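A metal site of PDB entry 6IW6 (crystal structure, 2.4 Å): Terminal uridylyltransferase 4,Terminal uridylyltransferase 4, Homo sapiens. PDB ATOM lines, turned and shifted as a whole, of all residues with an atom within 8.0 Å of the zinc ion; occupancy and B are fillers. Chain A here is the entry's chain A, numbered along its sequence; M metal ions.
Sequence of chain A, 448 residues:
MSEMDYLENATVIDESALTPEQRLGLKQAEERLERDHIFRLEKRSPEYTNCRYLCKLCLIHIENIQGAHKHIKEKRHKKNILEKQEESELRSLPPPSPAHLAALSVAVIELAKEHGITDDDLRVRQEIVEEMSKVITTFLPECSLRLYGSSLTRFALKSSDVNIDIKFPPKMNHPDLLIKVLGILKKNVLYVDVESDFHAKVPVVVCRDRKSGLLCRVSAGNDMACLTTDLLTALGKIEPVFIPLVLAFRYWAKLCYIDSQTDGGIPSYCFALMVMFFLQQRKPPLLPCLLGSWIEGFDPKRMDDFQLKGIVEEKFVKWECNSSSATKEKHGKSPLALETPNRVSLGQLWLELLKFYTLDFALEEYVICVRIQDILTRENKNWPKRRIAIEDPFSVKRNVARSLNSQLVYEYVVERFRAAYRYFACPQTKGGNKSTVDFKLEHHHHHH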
ATOM      1  N   ASP A  36      16.217  18.028  -7.193  1.00  0.00           N
ATOM      2  CA  ASP A  36      15.761  19.072  -6.282  1.00  0.00           C
ATOM      3  C   ASP A  36      16.886  20.016  -5.880  1.00  0.00           C
ATOM      4  O   ASP A  36      16.792  20.667  -4.833  1.00  0.00           O
ATOM      5  CB  ASP A  36      15.103  18.463  -5.046  1.00  0.00           C
ATOM      6  CG  ASP A  36      13.698  17.966  -5.326  1.00  0.00           C
ATOM      7  OD1 ASP A  36      12.827  18.797  -5.670  1.00  0.00           O
ATOM      8  OD2 ASP A  36      13.461  16.754  -5.199  1.00  0.00           O
ATOM      9  N   HIS A  37      17.955  20.097  -6.693  1.00  0.00           N
ATOM     10  CA  HIS A  37      19.066  21.045  -6.553  1.00  0.00           C
ATOM     11  C   HIS A  37      20.077  20.661  -5.473  1.00  0.00           C
ATOM     12  O   HIS A  37      20.851  21.517  -5.025  1.00  0.00           O
ATOM     13  CB  HIS A  37      18.586  22.474  -6.273  1.00  0.00           C
ATOM     14  CG  HIS A  37      17.480  22.933  -7.181  1.00  0.00           C
ATOM     15  ND1 HIS A  37      17.710  23.465  -8.433  1.00  0.00           N
ATOM     16  CD2 HIS A  37      16.141  22.946  -7.010  1.00  0.00           C
ATOM     17  CE1 HIS A  37      16.558  23.785  -8.990  1.00  0.00           C
ATOM     18  NE2 HIS A  37      15.589  23.469  -8.150  1.00  0.00           N
ATOM     19  N   ILE A  38      20.111  19.396  -5.051  1.00  0.00           N
ATOM     20  CA  ILE A  38      20.968  18.961  -3.950  1.00  0.00           C
ATOM     21  C   ILE A  38      22.077  18.076  -4.501  1.00  0.00           C
ATOM     22  O   ILE A  38      21.806  17.074  -5.172  1.00  0.00           O
ATOM     23  CB  ILE A  38      20.142  18.226  -2.879  1.00  0.00           C
ATOM     24  CG1 ILE A  38      19.172  19.224  -2.236  1.00  0.00           C
ATOM     25  CG2 ILE A  38      21.040  17.570  -1.846  1.00  0.00           C
ATOM     26  CD1 ILE A  38      18.064  18.569  -1.451  1.00  0.00           C
ATOM     27  N   LEU A  54      25.270  20.066  -0.657  1.00  0.00           N
ATOM     28  CA  LEU A  54      24.918  21.474  -0.824  1.00  0.00           C
ATOM     29  C   LEU A  54      23.615  21.542  -1.603  1.00  0.00           C
ATOM     30  O   LEU A  54      23.466  20.886  -2.635  1.00  0.00           O
ATOM     31  CB  LEU A  54      26.021  22.237  -1.559  1.00  0.00           C
ATOM     32  CG  LEU A  54      25.986  23.777  -1.585  1.00  0.00           C
ATOM     33  CD1 LEU A  54      25.254  24.293  -2.803  1.00  0.00           C
ATOM     34  CD2 LEU A  54      25.345  24.320  -0.327  1.00  0.00           C
ATOM     35  N   CYS A  55      22.658  22.310  -1.084  1.00  0.00           N
ATOM     36  CA  CYS A  55      21.487  22.709  -1.836  1.00  0.00           C
ATOM     37  C   CYS A  55      21.805  24.026  -2.523  1.00  0.00           C
ATOM     38  O   CYS A  55      22.010  25.057  -1.854  1.00  0.00           O
ATOM     39  CB  CYS A  55      20.248  22.842  -0.954  1.00  0.00           C
ATOM     40  SG  CYS A  55      18.859  23.497  -1.912  1.00  0.00           S
ATOM     41  N   LYS A  56      21.886  23.980  -3.873  1.00  0.00           N
ATOM     42  CA  LYS A  56      22.230  25.152  -4.671  1.00  0.00           C
ATOM     43  C   LYS A  56      21.098  26.169  -4.679  1.00  0.00           C
ATOM     44  O   LYS A  56      21.342  27.362  -4.860  1.00  0.00           O
ATOM     45  CB  LYS A  56      22.577  24.726  -6.104  1.00  0.00           C
ATOM     46  CG  LYS A  56      23.660  23.671  -6.203  1.00  0.00           C
ATOM     47  CD  LYS A  56      24.047  23.387  -7.648  1.00  0.00           C
ATOM     48  CE  LYS A  56      24.607  24.626  -8.329  1.00  0.00           C
ATOM     49  NZ  LYS A  56      25.140  24.321  -9.698  1.00  0.00           N
ATOM     50  N   LEU A  57      19.851  25.708  -4.525  1.00  0.00           N
ATOM     51  CA  LEU A  57      18.737  26.637  -4.408  1.00  0.00           C
ATOM     52  C   LEU A  57      18.899  27.498  -3.163  1.00  0.00           C
ATOM     53  O   LEU A  57      19.052  28.724  -3.256  1.00  0.00           O
ATOM     54  CB  LEU A  57      17.418  25.861  -4.349  1.00  0.00           C
ATOM     55  CG  LEU A  57      16.120  26.649  -4.155  1.00  0.00           C
ATOM     56  CD1 LEU A  57      15.897  27.580  -5.330  1.00  0.00           C
ATOM     57  CD2 LEU A  57      14.913  25.735  -3.956  1.00  0.00           C
ATOM     58  N   CYS A  58      18.872  26.872  -1.990  1.00  0.00           N
ATOM     59  CA  CYS A  58      18.934  27.604  -0.737  1.00  0.00           C
ATOM     60  C   CYS A  58      20.353  27.973  -0.318  1.00  0.00           C
ATOM     61  O   CYS A  58      20.530  28.694   0.668  1.00  0.00           O
ATOM     62  CB  CYS A  58      18.274  26.784   0.381  1.00  0.00           C
ATOM     63  SG  CYS A  58      16.598  26.244   0.038  1.00  0.00           S
ATOM     64  N   LEU A  59      21.362  27.515  -1.062  1.00  0.00           N
ATOM     65  CA  LEU A  59      22.759  27.619  -0.634  1.00  0.00           C
ATOM     66  C   LEU A  59      22.917  27.120   0.802  1.00  0.00           C
ATOM     67  O   LEU A  59      23.465  27.810   1.665  1.00  0.00           O
ATOM     68  CB  LEU A  59      23.288  29.051  -0.794  1.00  0.00           C
ATOM     69  CG  LEU A  59      23.406  29.665  -2.197  1.00  0.00           C
ATOM     70  CD1 LEU A  59      23.802  31.134  -2.128  1.00  0.00           C
ATOM     71  CD2 LEU A  59      24.364  28.890  -3.097  1.00  0.00           C
ATOM     72  N   ILE A  60      22.417  25.919   1.055  1.00  0.00           N
ATOM     73  CA  ILE A  60      22.375  25.388   2.417  1.00  0.00           C
ATOM     74  C   ILE A  60      23.168  24.088   2.474  1.00  0.00           C
ATOM     75  O   ILE A  60      23.010  23.219   1.609  1.00  0.00           O
ATOM     76  CB  ILE A  60      20.931  25.169   2.916  1.00  0.00           C
ATOM     77  CG1 ILE A  60      20.254  26.518   3.113  1.00  0.00           C
ATOM     78  CG2 ILE A  60      20.932  24.427   4.243  1.00  0.00           C
ATOM     79  CD1 ILE A  60      21.101  27.496   3.884  1.00  0.00           C
ATOM     80  N   ILE A  62      23.684  20.520   3.864  1.00  0.00           N
ATOM     81  CA  ILE A  62      22.886  19.419   4.384  1.00  0.00           C
ATOM     82  C   ILE A  62      23.814  18.249   4.650  1.00  0.00           C
ATOM     83  O   ILE A  62      24.725  17.972   3.856  1.00  0.00           O
ATOM     84  CB  ILE A  62      21.757  19.040   3.401  1.00  0.00           C
ATOM     85  CG1 ILE A  62      20.796  20.224   3.211  1.00  0.00           C
ATOM     86  CG2 ILE A  62      21.014  17.813   3.901  1.00  0.00           C
ATOM     87  CD1 ILE A  62      19.961  20.147   1.954  1.00  0.00           C
ATOM     88  N   ALA A  68      18.466  15.668   3.506  1.00  0.00           N
ATOM     89  CA  ALA A  68      18.162  16.304   2.229  1.00  0.00           C
ATOM     90  C   ALA A  68      16.689  16.115   1.881  1.00  0.00           C
ATOM     91  O   ALA A  68      16.041  17.062   1.400  1.00  0.00           O
ATOM     92  CB  ALA A  68      19.061  15.724   1.128  1.00  0.00           C
ATOM     93  N   HIS A  71      14.731  18.421   3.960  1.00  0.00           N
ATOM     94  CA  HIS A  71      14.937  19.817   3.586  1.00  0.00           C
ATOM     95  C   HIS A  71      14.122  20.184   2.341  1.00  0.00           C
ATOM     96  O   HIS A  71      13.584  21.288   2.255  1.00  0.00           O
ATOM     97  CB  HIS A  71      16.425  20.074   3.352  1.00  0.00           C
ATOM     98  CG  HIS A  71      16.727  21.394   2.714  1.00  0.00           C
ATOM     99  ND1 HIS A  71      16.945  22.546   3.434  1.00  0.00           N
ATOM    100  CD2 HIS A  71      16.860  21.746   1.408  1.00  0.00           C
ATOM    101  CE1 HIS A  71      17.187  23.542   2.613  1.00  0.00           C
ATOM    102  NE2 HIS A  71      17.139  23.082   1.373  1.00  0.00           N
ATOM    103  N   ILE A  72      14.062  19.261   1.370  1.00  0.00           N
ATOM    104  CA  ILE A  72      13.282  19.497   0.148  1.00  0.00           C
ATOM    105  C   ILE A  72      11.863  19.941   0.484  1.00  0.00           C
ATOM    106  O   ILE A  72      11.293  20.807  -0.192  1.00  0.00           O
ATOM    107  CB  ILE A  72      13.277  18.221  -0.715  1.00  0.00           C
ATOM    108  CG1 ILE A  72      14.624  18.033  -1.412  1.00  0.00           C
ATOM    109  CG2 ILE A  72      12.153  18.250  -1.729  1.00  0.00           C
ATOM    110  CD1 ILE A  72      14.760  16.669  -2.061  1.00  0.00           C
ATOM    111  N   LYS A  73      11.281  19.374   1.533  1.00  0.00           N
ATOM    112  CA  LYS A  73       9.896  19.607   1.876  1.00  0.00           C
ATOM    113  C   LYS A  73       9.710  20.622   2.995  1.00  0.00           C
ATOM    114  O   LYS A  73       8.594  20.772   3.497  1.00  0.00           O
ATOM    115  CB  LYS A  73       9.217  18.284   2.242  1.00  0.00           C
ATOM    116  CG  LYS A  73       9.088  17.319   1.079  1.00  0.00           C
ATOM    117  CD  LYS A  73       7.998  17.776   0.123  1.00  0.00           C
ATOM    118  CE  LYS A  73       6.629  17.690   0.796  1.00  0.00           C
ATOM    119  NZ  LYS A  73       5.581  18.455   0.059  1.00  0.00           N
ATOM    120  N   GLU A  74      10.764  21.326   3.394  1.00  0.00           N
ATOM    121  CA  GLU A  74      10.696  22.258   4.506  1.00  0.00           C
ATOM    122  C   GLU A  74      10.434  23.686   4.001  1.00  0.00           C
ATOM    123  O   GLU A  74      10.200  23.921   2.806  1.00  0.00           O
ATOM    124  CB  GLU A  74      11.966  22.161   5.344  1.00  0.00           C
ATOM    125  CG  GLU A  74      11.812  21.239   6.552  1.00  0.00           C
ATOM    126  CD  GLU A  74      13.136  20.721   7.089  1.00  0.00           C
ATOM    127  OE1 GLU A  74      13.129  19.736   7.864  1.00  0.00           O
ATOM    128  OE2 GLU A  74      14.189  21.309   6.736  1.00  0.00           O
ATOM    129  N   LYS A  75      10.483  24.652   4.916  1.00  0.00           N
ATOM    130  CA  LYS A  75      10.027  26.009   4.605  1.00  0.00           C
ATOM    131  C   LYS A  75      10.960  26.706   3.617  1.00  0.00           C
ATOM    132  O   LYS A  75      10.509  27.218   2.593  1.00  0.00           O
ATOM    133  CB  LYS A  75       9.909  26.829   5.883  1.00  0.00           C
ATOM    134  CG  LYS A  75       8.580  26.700   6.599  1.00  0.00           C
ATOM    135  CD  LYS A  75       8.569  27.513   7.888  1.00  0.00           C
ATOM    136  CE  LYS A  75       7.237  27.362   8.630  1.00  0.00           C
ATOM    137  NZ  LYS A  75       6.117  27.999   7.889  1.00  0.00           N
ATOM    138  N   ARG A  76      12.249  26.749   3.934  1.00  0.00           N
ATOM    139  CA  ARG A  76      13.200  27.512   3.125  1.00  0.00           C
ATOM    140  C   ARG A  76      13.165  27.046   1.668  1.00  0.00           C
ATOM    141  O   ARG A  76      13.077  27.865   0.744  1.00  0.00           O
ATOM    142  CB  ARG A  76      14.604  27.379   3.697  1.00  0.00           C
ATOM    143  CG  ARG A  76      15.459  28.639   3.584  1.00  0.00           C
ATOM    144  CD  ARG A  76      16.733  28.508   4.409  1.00  0.00           C
ATOM    145  NE  ARG A  76      17.328  29.812   4.703  1.00  0.00           N
ATOM    146  CZ  ARG A  76      16.891  30.624   5.666  1.00  0.00           C
ATOM    147  NH1 ARG A  76      15.857  30.268   6.429  1.00  0.00           N
ATOM    148  NH2 ARG A  76      17.491  31.787   5.872  1.00  0.00           N
ATOM    149  N   HIS A  77      13.222  25.730   1.449  1.00  0.00           N
ATOM    150  CA  HIS A  77      13.258  25.206   0.088  1.00  0.00           C
ATOM    151  C   HIS A  77      11.955  25.495  -0.655  1.00  0.00           C
ATOM    152  O   HIS A  77      11.973  25.856  -1.838  1.00  0.00           O
ATOM    153  CB  HIS A  77      13.527  23.703   0.124  1.00  0.00           C
ATOM    154  CG  HIS A  77      13.944  23.136  -1.192  1.00  0.00           C
ATOM    155  ND1 HIS A  77      15.241  23.250  -1.671  1.00  0.00           N
ATOM    156  CD2 HIS A  77      13.249  22.454  -2.126  1.00  0.00           C
ATOM    157  CE1 HIS A  77      15.318  22.663  -2.848  1.00  0.00           C
ATOM    158  NE2 HIS A  77      14.127  22.166  -3.146  1.00  0.00           N
ATOM    159  N   LYS A  78      10.812  25.331   0.018  1.00  0.00           N
ATOM    160  CA  LYS A  78       9.530  25.629  -0.624  1.00  0.00           C
ATOM    161  C   LYS A  78       9.448  27.092  -1.030  1.00  0.00           C
ATOM    162  O   LYS A  78       9.076  27.424  -2.162  1.00  0.00           O
ATOM    163  CB  LYS A  78       8.386  25.255   0.319  1.00  0.00           C
ATOM    164  CG  LYS A  78       8.006  23.782   0.292  1.00  0.00           C
ATOM    165  CD  LYS A  78       6.769  23.525   1.151  1.00  0.00           C
ATOM    166  CE  LYS A  78       6.113  22.186   0.821  1.00  0.00           C
ATOM    167  NZ  LYS A  78       5.488  22.180  -0.532  1.00  0.00           N
ATOM    168  N   ASN A  80      11.854  29.161  -1.633  1.00  0.00           N
ATOM    169  CA  ASN A  80      12.767  29.489  -2.724  1.00  0.00           C
ATOM    170  C   ASN A  80      12.260  28.963  -4.050  1.00  0.00           C
ATOM    171  O   ASN A  80      12.386  29.632  -5.083  1.00  0.00           O
ATOM    172  CB  ASN A  80      14.165  28.960  -2.423  1.00  0.00           C
ATOM    173  CG  ASN A  80      14.887  29.784  -1.391  1.00  0.00           C
ATOM    174  OD1 ASN A  80      14.267  30.456  -0.571  1.00  0.00           O
ATOM    175  ND2 ASN A  80      16.216  29.766  -1.444  1.00  0.00           N
ATOM    176  N   ILE A  81      11.683  27.753  -4.053  1.00  0.00           N
ATOM    177  CA  ILE A  81      11.040  27.233  -5.249  1.00  0.00           C
ATOM    178  C   ILE A  81       9.991  28.226  -5.750  1.00  0.00           C
ATOM    179  O   ILE A  81       9.927  28.555  -6.945  1.00  0.00           O
ATOM    180  CB  ILE A  81      10.421  25.845  -4.967  1.00  0.00           C
ATOM    181  CG1 ILE A  81      11.501  24.772  -4.897  1.00  0.00           C
ATOM    182  CG2 ILE A  81       9.366  25.505  -6.009  1.00  0.00           C
ATOM    183  CD1 ILE A  81      12.145  24.472  -6.234  1.00  0.00           C
HETATM  184 ZN    ZN M   1      16.923  23.953  -0.701  1.00  0.00          ZN
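Of the 22 residues printed, 4 come within 4 Å of the zinc ion.
A ring nitrogen (ND1) of His 77 is bound to the zinc ion, at 2.1 Å. A ring nitrogen (NE2) of His 71 binds the zinc ion (2.3 Å). The side-chain sulfur (SG) of Cys 55 is bound to the zinc ion, 2.3 Å away. The zinc ion is bound by SG of Cys 58.
The side-chain sulfur (SG) of Cys 55 lies close to the backbone NH (N) of Leu 57 (3.6 Å). The backbone NH (N) of Cys 55 lies within hydrogen-bond range of the backbone carbonyl oxygen (O) of Ile 60, at 2.9 Å. A ring nitrogen (NE2) of His 77 sits close to the backbone carbonyl oxygen (O) of Asp 36.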
